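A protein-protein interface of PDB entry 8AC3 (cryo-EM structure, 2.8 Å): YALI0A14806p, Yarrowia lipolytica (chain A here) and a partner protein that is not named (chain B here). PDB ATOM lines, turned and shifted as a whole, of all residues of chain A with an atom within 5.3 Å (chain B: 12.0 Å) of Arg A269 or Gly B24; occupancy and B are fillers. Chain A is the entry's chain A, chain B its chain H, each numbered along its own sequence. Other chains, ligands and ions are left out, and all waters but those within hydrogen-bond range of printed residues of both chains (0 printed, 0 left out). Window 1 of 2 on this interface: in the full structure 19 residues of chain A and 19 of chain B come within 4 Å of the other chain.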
ATOM      1  N   GLU A 267     -13.008  27.829  -8.195  1.00  0.00           N
ATOM      2  CA  GLU A 267     -13.273  26.485  -7.732  1.00  0.00           C
ATOM      3  C   GLU A 267     -12.012  25.908  -7.115  1.00  0.00           C
ATOM      4  O   GLU A 267     -10.914  26.233  -7.556  1.00  0.00           O
ATOM      5  CB  GLU A 267     -13.855  25.714  -8.907  1.00  0.00           C
ATOM      6  CG  GLU A 267     -13.211  24.405  -9.196  1.00  0.00           C
ATOM      7  CD  GLU A 267     -13.300  24.116 -10.683  1.00  0.00           C
ATOM      8  OE1 GLU A 267     -14.391  24.299 -11.269  1.00  0.00           O
ATOM      9  OE2 GLU A 267     -12.271  23.722 -11.250  1.00  0.00           O
ATOM     10  N   VAL A 268     -12.198  25.106  -6.068  1.00  0.00           N
ATOM     11  CA  VAL A 268     -11.127  24.317  -5.500  1.00  0.00           C
ATOM     12  C   VAL A 268     -11.566  22.871  -5.589  1.00  0.00           C
ATOM     13  O   VAL A 268     -12.645  22.541  -5.119  1.00  0.00           O
ATOM     14  CB  VAL A 268     -10.885  24.693  -4.031  1.00  0.00           C
ATOM     15  CG1 VAL A 268      -9.790  23.835  -3.427  1.00  0.00           C
ATOM     16  CG2 VAL A 268     -10.570  26.172  -3.877  1.00  0.00           C
ATOM     17  N   ARG A 269     -10.746  22.025  -6.201  1.00  0.00           N
ATOM     18  CA  ARG A 269     -11.068  20.614  -6.199  1.00  0.00           C
ATOM     19  C   ARG A 269     -10.020  19.865  -5.404  1.00  0.00           C
ATOM     20  O   ARG A 269      -8.828  19.972  -5.678  1.00  0.00           O
ATOM     21  CB  ARG A 269     -11.000  20.055  -7.610  1.00  0.00           C
ATOM     22  CG  ARG A 269     -12.064  20.613  -8.518  1.00  0.00           C
ATOM     23  CD  ARG A 269     -11.698  20.066  -9.882  1.00  0.00           C
ATOM     24  NE  ARG A 269     -12.654  20.828 -10.644  1.00  0.00           N
ATOM     25  CZ  ARG A 269     -13.845  20.414 -11.059  1.00  0.00           C
ATOM     26  NH1 ARG A 269     -14.257  19.174 -10.848  1.00  0.00           N
ATOM     27  NH2 ARG A 269     -14.611  21.281 -11.690  1.00  0.00           N
ATOM     28  N   LEU A 270     -10.487  19.084  -4.437  1.00  0.00           N
ATOM     29  CA  LEU A 270      -9.592  18.339  -3.584  1.00  0.00           C
ATOM     30  C   LEU A 270      -9.974  16.890  -3.770  1.00  0.00           C
ATOM     31  O   LEU A 270     -10.627  16.301  -2.919  1.00  0.00           O
ATOM     32  CB  LEU A 270      -9.841  18.789  -2.149  1.00  0.00           C
ATOM     33  CG  LEU A 270      -9.676  20.286  -1.907  1.00  0.00           C
ATOM     34  CD1 LEU A 270     -10.358  20.710  -0.613  1.00  0.00           C
ATOM     35  CD2 LEU A 270      -8.205  20.654  -1.867  1.00  0.00           C
ATOM     36  N   ARG A 271      -9.642  16.373  -4.940  1.00  0.00           N
ATOM     37  CA  ARG A 271     -10.058  15.028  -5.253  1.00  0.00           C
ATOM     38  C   ARG A 271      -9.299  14.039  -4.372  1.00  0.00           C
ATOM     39  O   ARG A 271      -8.107  14.202  -4.135  1.00  0.00           O
ATOM     40  CB  ARG A 271      -9.833  14.781  -6.736  1.00  0.00           C
ATOM     41  CG  ARG A 271     -10.020  13.334  -7.129  1.00  0.00           C
ATOM     42  CD  ARG A 271     -10.286  13.397  -8.607  1.00  0.00           C
ATOM     43  NE  ARG A 271     -10.195  12.025  -9.068  1.00  0.00           N
ATOM     44  CZ  ARG A 271     -10.169  11.653 -10.339  1.00  0.00           C
ATOM     45  NH1 ARG A 271     -10.237  12.550 -11.310  1.00  0.00           N
ATOM     46  NH2 ARG A 271     -10.070  10.372 -10.634  1.00  0.00           N
ATOM     47  N   LEU A 450     -17.020  27.177  -5.864  1.00  0.00           N
ATOM     48  CA  LEU A 450     -17.370  25.776  -5.850  1.00  0.00           C
ATOM     49  C   LEU A 450     -16.234  25.024  -5.180  1.00  0.00           C
ATOM     50  O   LEU A 450     -15.075  25.235  -5.506  1.00  0.00           O
ATOM     51  CB  LEU A 450     -17.488  25.392  -7.318  1.00  0.00           C
ATOM     52  CG  LEU A 450     -17.457  23.898  -7.593  1.00  0.00           C
ATOM     53  CD1 LEU A 450     -18.789  23.279  -7.236  1.00  0.00           C
ATOM     54  CD2 LEU A 450     -17.194  23.666  -9.068  1.00  0.00           C
ATOM     55  N   GLY A 452     -15.090  21.053  -4.126  1.00  0.00           N
ATOM     56  CA  GLY A 452     -15.429  19.649  -4.109  1.00  0.00           C
ATOM     57  C   GLY A 452     -14.323  18.876  -3.419  1.00  0.00           C
ATOM     58  O   GLY A 452     -13.143  19.146  -3.624  1.00  0.00           O
ATOM     59  N   ILE A 456     -14.646  13.143  -6.714  1.00  0.00           N
ATOM     60  CA  ILE A 456     -15.414  14.122  -7.465  1.00  0.00           C
ATOM     61  C   ILE A 456     -15.009  14.083  -8.935  1.00  0.00           C
ATOM     62  O   ILE A 456     -15.177  15.072  -9.642  1.00  0.00           O
ATOM     63  CB  ILE A 456     -15.178  15.514  -6.859  1.00  0.00           C
ATOM     64  CG1 ILE A 456     -13.670  15.771  -6.803  1.00  0.00           C
ATOM     65  CG2 ILE A 456     -15.839  15.613  -5.490  1.00  0.00           C
ATOM     66  CD1 ILE A 456     -13.252  17.199  -6.527  1.00  0.00           C
ATOM     67  N   LEU A 459     -17.588  15.359 -11.164  1.00  0.00           N
ATOM     68  CA  LEU A 459     -18.033  16.737 -11.110  1.00  0.00           C
ATOM     69  C   LEU A 459     -17.427  17.426 -12.324  1.00  0.00           C
ATOM     70  O   LEU A 459     -16.223  17.322 -12.520  1.00  0.00           O
ATOM     71  CB  LEU A 459     -17.503  17.315  -9.801  1.00  0.00           C
ATOM     72  CG  LEU A 459     -17.777  18.791  -9.553  1.00  0.00           C
ATOM     73  CD1 LEU A 459     -19.264  19.034  -9.420  1.00  0.00           C
ATOM     74  CD2 LEU A 459     -17.048  19.254  -8.300  1.00  0.00           C
ATOM     75  N   TYR A 460     -18.249  18.047 -13.179  1.00  0.00           N
ATOM     76  CA  TYR A 460     -17.696  18.657 -14.383  1.00  0.00           C
ATOM     77  C   TYR A 460     -16.884  19.892 -14.024  1.00  0.00           C
ATOM     78  O   TYR A 460     -16.953  20.367 -12.900  1.00  0.00           O
ATOM     79  CB  TYR A 460     -18.796  19.059 -15.362  1.00  0.00           C
ATOM     80  CG  TYR A 460     -19.524  17.882 -15.949  1.00  0.00           C
ATOM     81  CD1 TYR A 460     -18.834  16.739 -16.332  1.00  0.00           C
ATOM     82  CD2 TYR A 460     -20.903  17.900 -16.096  1.00  0.00           C
ATOM     83  CE1 TYR A 460     -19.501  15.638 -16.846  1.00  0.00           C
ATOM     84  CE2 TYR A 460     -21.585  16.810 -16.622  1.00  0.00           C
ATOM     85  CZ  TYR A 460     -20.879  15.674 -16.989  1.00  0.00           C
ATOM     86  OH  TYR A 460     -21.533  14.596 -17.509  1.00  0.00           O
ATOM     87  N   ASP A 461     -16.164  20.417 -15.011  1.00  0.00           N
ATOM     88  CA  ASP A 461     -15.364  21.625 -14.888  1.00  0.00           C
ATOM     89  C   ASP A 461     -16.230  22.854 -14.583  1.00  0.00           C
ATOM     90  O   ASP A 461     -17.458  22.835 -14.700  1.00  0.00           O
ATOM     91  CB  ASP A 461     -14.581  21.792 -16.189  1.00  0.00           C
ATOM     92  CG  ASP A 461     -15.493  21.549 -17.381  1.00  0.00           C
ATOM     93  OD1 ASP A 461     -16.456  22.327 -17.525  1.00  0.00           O
ATOM     94  OD2 ASP A 461     -15.262  20.560 -18.129  1.00  0.00           O
ATOM     95  N   TYR A 462     -15.562  23.944 -14.207  1.00  0.00           N
ATOM     96  CA  TYR A 462     -16.243  25.157 -13.807  1.00  0.00           C
ATOM     97  C   TYR A 462     -17.272  25.625 -14.832  1.00  0.00           C
ATOM     98  O   TYR A 462     -18.376  25.961 -14.425  1.00  0.00           O
ATOM     99  CB  TYR A 462     -15.250  26.276 -13.517  1.00  0.00           C
ATOM    100  CG  TYR A 462     -15.897  27.463 -12.866  1.00  0.00           C
ATOM    101  CD1 TYR A 462     -16.023  27.533 -11.486  1.00  0.00           C
ATOM    102  CD2 TYR A 462     -16.400  28.510 -13.626  1.00  0.00           C
ATOM    103  CE1 TYR A 462     -16.613  28.634 -10.874  1.00  0.00           C
ATOM    104  CE2 TYR A 462     -17.010  29.606 -13.026  1.00  0.00           C
ATOM    105  CZ  TYR A 462     -17.117  29.675 -11.643  1.00  0.00           C
ATOM    106  OH  TYR A 462     -17.706  30.764 -11.051  1.00  0.00           O
ATOM    107  N   TRP B  11     -17.430   9.400 -16.840  1.00  0.00           N
ATOM    108  CA  TRP B  11     -17.299  10.254 -15.675  1.00  0.00           C
ATOM    109  C   TRP B  11     -17.696   9.488 -14.422  1.00  0.00           C
ATOM    110  O   TRP B  11     -18.751   8.859 -14.366  1.00  0.00           O
ATOM    111  CB  TRP B  11     -18.215  11.447 -15.834  1.00  0.00           C
ATOM    112  CG  TRP B  11     -17.929  12.195 -17.084  1.00  0.00           C
ATOM    113  CD1 TRP B  11     -18.631  12.155 -18.251  1.00  0.00           C
ATOM    114  CD2 TRP B  11     -16.830  13.090 -17.287  1.00  0.00           C
ATOM    115  NE1 TRP B  11     -18.053  12.994 -19.163  1.00  0.00           N
ATOM    116  CE2 TRP B  11     -16.944  13.572 -18.607  1.00  0.00           C
ATOM    117  CE3 TRP B  11     -15.762  13.515 -16.486  1.00  0.00           C
ATOM    118  CZ2 TRP B  11     -16.028  14.476 -19.140  1.00  0.00           C
ATOM    119  CZ3 TRP B  11     -14.854  14.407 -17.018  1.00  0.00           C
ATOM    120  CH2 TRP B  11     -14.990  14.877 -18.325  1.00  0.00           C
ATOM    121  N   GLY B  12     -16.844   9.568 -13.414  1.00  0.00           N
ATOM    122  CA  GLY B  12     -17.086   8.804 -12.210  1.00  0.00           C
ATOM    123  C   GLY B  12     -16.212   7.561 -12.155  1.00  0.00           C
ATOM    124  O   GLY B  12     -15.794   7.173 -11.067  1.00  0.00           O
ATOM    125  N   MET B  14     -13.427   6.811 -14.717  1.00  0.00           N
ATOM    126  CA  MET B  14     -12.712   7.062 -15.955  1.00  0.00           C
ATOM    127  C   MET B  14     -11.579   6.055 -16.129  1.00  0.00           C
ATOM    128  O   MET B  14     -11.210   5.740 -17.255  1.00  0.00           O
ATOM    129  CB  MET B  14     -12.111   8.468 -15.962  1.00  0.00           C
ATOM    130  CG  MET B  14     -11.755   8.965 -17.351  1.00  0.00           C
ATOM    131  SD  MET B  14     -13.244   9.199 -18.352  1.00  0.00           S
ATOM    132  CE  MET B  14     -14.009  10.523 -17.420  1.00  0.00           C
ATOM    133  N   GLN B  19      -6.370   9.043  -7.249  1.00  0.00           N
ATOM    134  CA  GLN B  19      -5.727  10.331  -7.091  1.00  0.00           C
ATOM    135  C   GLN B  19      -5.901  10.753  -5.649  1.00  0.00           C
ATOM    136  O   GLN B  19      -6.972  10.577  -5.074  1.00  0.00           O
ATOM    137  CB  GLN B  19      -6.383  11.365  -7.990  1.00  0.00           C
ATOM    138  CG  GLN B  19      -6.389  10.906  -9.426  1.00  0.00           C
ATOM    139  CD  GLN B  19      -6.710  12.041 -10.360  1.00  0.00           C
ATOM    140  OE1 GLN B  19      -6.744  13.209  -9.961  1.00  0.00           O
ATOM    141  NE2 GLN B  19      -6.960  11.694 -11.616  1.00  0.00           N
ATOM    142  N   LYS B  20      -4.826  11.257  -5.063  1.00  0.00           N
ATOM    143  CA  LYS B  20      -4.910  11.800  -3.729  1.00  0.00           C
ATOM    144  C   LYS B  20      -3.849  12.876  -3.634  1.00  0.00           C
ATOM    145  O   LYS B  20      -2.784  12.730  -4.209  1.00  0.00           O
ATOM    146  CB  LYS B  20      -4.673  10.678  -2.723  1.00  0.00           C
ATOM    147  CG  LYS B  20      -4.975  11.084  -1.296  1.00  0.00           C
ATOM    148  CD  LYS B  20      -5.041   9.912  -0.361  1.00  0.00           C
ATOM    149  CE  LYS B  20      -5.012  10.330   1.091  1.00  0.00           C
ATOM    150  NZ  LYS B  20      -5.183   9.162   1.988  1.00  0.00           N
ATOM    151  N   GLY B  21      -4.152  13.974  -2.952  1.00  0.00           N
ATOM    152  CA  GLY B  21      -3.082  14.899  -2.631  1.00  0.00           C
ATOM    153  C   GLY B  21      -2.897  16.033  -3.635  1.00  0.00           C
ATOM    154  O   GLY B  21      -2.072  16.908  -3.402  1.00  0.00           O
ATOM    155  N   ILE B  22      -3.699  16.078  -4.700  1.00  0.00           N
ATOM    156  CA  ILE B  22      -3.592  17.207  -5.606  1.00  0.00           C
ATOM    157  C   ILE B  22      -4.745  18.167  -5.349  1.00  0.00           C
ATOM    158  O   ILE B  22      -5.901  17.768  -5.429  1.00  0.00           O
ATOM    159  CB  ILE B  22      -3.602  16.742  -7.069  1.00  0.00           C
ATOM    160  CG1 ILE B  22      -2.599  15.617  -7.321  1.00  0.00           C
ATOM    161  CG2 ILE B  22      -3.366  17.934  -7.979  1.00  0.00           C
ATOM    162  CD1 ILE B  22      -2.860  14.844  -8.600  1.00  0.00           C
ATOM    163  N   ALA B  23      -4.432  19.440  -5.099  1.00  0.00           N
ATOM    164  CA  ALA B  23      -5.461  20.458  -4.994  1.00  0.00           C
ATOM    165  C   ALA B  23      -5.433  21.263  -6.280  1.00  0.00           C
ATOM    166  O   ALA B  23      -4.364  21.700  -6.687  1.00  0.00           O
ATOM    167  CB  ALA B  23      -5.176  21.333  -3.803  1.00  0.00           C
ATOM    168  N   GLY B  24      -6.591  21.425  -6.918  1.00  0.00           N
ATOM    169  CA  GLY B  24      -6.665  22.173  -8.161  1.00  0.00           C
ATOM    170  C   GLY B  24      -7.454  23.453  -7.938  1.00  0.00           C
ATOM    171  O   GLY B  24      -8.451  23.438  -7.231  1.00  0.00           O
ATOM    172  N   TYR B  25      -6.988  24.555  -8.512  1.00  0.00           N
ATOM    173  CA  TYR B  25      -7.672  25.814  -8.313  1.00  0.00           C
ATOM    174  C   TYR B  25      -7.869  26.484  -9.654  1.00  0.00           C
ATOM    175  O   TYR B  25      -6.975  26.461 -10.494  1.00  0.00           O
ATOM    176  CB  TYR B  25      -6.770  26.756  -7.533  1.00  0.00           C
ATOM    177  CG  TYR B  25      -6.369  26.180  -6.212  1.00  0.00           C
ATOM    178  CD1 TYR B  25      -5.331  25.260  -6.119  1.00  0.00           C
ATOM    179  CD2 TYR B  25      -7.044  26.546  -5.055  1.00  0.00           C
ATOM    180  CE1 TYR B  25      -4.950  24.752  -4.891  1.00  0.00           C
ATOM    181  CE2 TYR B  25      -6.697  26.019  -3.824  1.00  0.00           C
ATOM    182  CZ  TYR B  25      -5.638  25.131  -3.747  1.00  0.00           C
ATOM    183  OH  TYR B  25      -5.271  24.620  -2.546  1.00  0.00           O
ATOM    184  N   THR B  26      -9.026  27.113  -9.840  1.00  0.00           N
ATOM    185  CA  THR B  26      -9.152  27.959 -11.005  1.00  0.00           C
ATOM    186  C   THR B  26     -10.142  29.080 -10.749  1.00  0.00           C
ATOM    187  O   THR B  26     -10.893  29.034  -9.792  1.00  0.00           O
ATOM    188  CB  THR B  26      -9.522  27.148 -12.248  1.00  0.00           C
ATOM    189  OG1 THR B  26      -9.263  28.057 -13.318  1.00  0.00           O
ATOM    190  CG2 THR B  26     -10.960  26.677 -12.247  1.00  0.00           C
ATOM    191  N   ILE B  27     -10.162  30.071 -11.635  1.00  0.00           N
ATOM    192  CA  ILE B  27     -11.123  31.145 -11.480  1.00  0.00           C
ATOM    193  C   ILE B  27     -12.083  31.175 -12.663  1.00  0.00           C
ATOM    194  O   ILE B  27     -11.778  30.662 -13.739  1.00  0.00           O
ATOM    195  CB  ILE B  27     -10.395  32.476 -11.278  1.00  0.00           C
ATOM    196  CG1 ILE B  27      -9.499  32.781 -12.478  1.00  0.00           C
ATOM    197  CG2 ILE B  27      -9.611  32.437  -9.976  1.00  0.00           C
ATOM    198  CD1 ILE B  27      -9.013  34.211 -12.544  1.00  0.00           C
ATOM    199  N   SER B  28     -13.235  31.814 -12.438  1.00  0.00           N
ATOM    200  CA  SER B  28     -14.315  31.975 -13.395  1.00  0.00           C
ATOM    201  C   SER B  28     -13.827  32.657 -14.669  1.00  0.00           C
ATOM    202  O   SER B  28     -12.997  33.558 -14.607  1.00  0.00           O
ATOM    203  CB  SER B  28     -15.381  32.814 -12.768  1.00  0.00           C
ATOM    204  OG  SER B  28     -16.407  33.089 -13.704  1.00  0.00           O
ATOM    205  N   PRO B  29     -14.365  32.298 -15.856  1.00  0.00           N
ATOM    206  CA  PRO B  29     -14.075  33.040 -17.078  1.00  0.00           C
ATOM    207  C   PRO B  29     -14.440  34.512 -16.954  1.00  0.00           C
ATOM    208  O   PRO B  29     -13.766  35.342 -17.549  1.00  0.00           O
ATOM    209  CB  PRO B  29     -14.939  32.380 -18.158  1.00  0.00           C
ATOM    210  CG  PRO B  29     -15.970  31.591 -17.385  1.00  0.00           C
ATOM    211  CD  PRO B  29     -15.280  31.174 -16.103  1.00  0.00           C
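O of Thr B26 sits at hydrogen-bond distance from N of Glu A267 (2.9 Å).
N of Arg A269 lies within hydrogen-bond range of O of Gly B24 (2.9 Å).
NE2 of Gln B19 lies close to NH1 of Arg A271 (3.4 Å).
The side-chain carboxylate (OE1) of Glu A267 sits close to the backbone NH (N) of Tyr A462, 3.2 Å away.
O of Leu A450 lies within hydrogen-bond range of N of Val A268 (2.9 Å).
The backbone NH (N) of Gly A452 is in hydrogen-bond range of the backbone carbonyl oxygen (O) of Val A268, 3.0 Å away.
The guanidinium group (NH1) of Arg A269 sits at hydrogen-bond distance from the backbone carbonyl oxygen (O) of Leu A459 (3.2 Å).
NH2 of Arg A269 lies within hydrogen-bond range of O of Tyr A460, 2.8 Å away.
O of Gly A452 sits at hydrogen-bond distance from N of Leu A270, at 2.8 Å.
Among the printed residues, pairs that only touch across the chains: Glu A267 with Gly B24 (3.7 Å), Glu A267 with Tyr B25 (3.4 Å), Val A268 with Gly B24 (3.3 Å), Val A268 with Tyr B25 (3.7 Å), Arg A269 with Ile B22 (3.7 Å), Arg A269 with Ala B23 (3.5 Å), Leu A270 with Ala B23 (3.7 Å), Tyr A460 with Trp B11 (3.7 Å), Tyr A462 with Ser B28 (3.5 Å) and Tyr A462 with Pro B29 (3.8 Å).
Arg A269 touches three residues of chain B.
Of the printed residues of chain B, Arg A271 touches Gln B19.
No residue of chain B comes within 4 Å of Gly A452.
No residue of chain B comes within 4 Å of Ile A456.
No residue of chain B comes within 4 Å of Leu A459.
Of the printed residues of chain B, Tyr A460 touches Trp B11.
No residue of chain B comes within 4 Å of Asp A461.
Of the printed residues of chain A, Gln B19 touches Arg A271.
Printed residues of chain A within 4 Å of Ala B23: Arg A269 (3.5 Å) and Leu A270 (3.7 Å).
Gly B24 touches just these residues of chain A: Glu A267, Val A268 and Arg A269.
The nearest residue of chain B that does not touch Arg A269 is Tyr B25 (5.1 Å).
Printed residues of chain A that touch a printed residue of chain B: Glu A267, Val A268, Arg A269, Leu A270, Arg A271, Tyr A460 and Tyr A462.
Of the 14 printed residues of chain B, 9 touch a printed residue of chain A.
Printed residues of chain B that touch a printed residue of chain A: Trp B11, Gln B19, Ile B22, Ala B23, Gly B24, Tyr B25, Thr B26, Ser B28 and Pro B29.
Hydrophobic or aromatic side chains of chain B that line the printed part of chain A: Trp B11, Ala B23, Tyr B25 and Pro B29.
Among the printed residues, no Asp or Glu carboxylate lies within 4 Å of a Lys or Arg side-chain nitrogen of the other chain.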
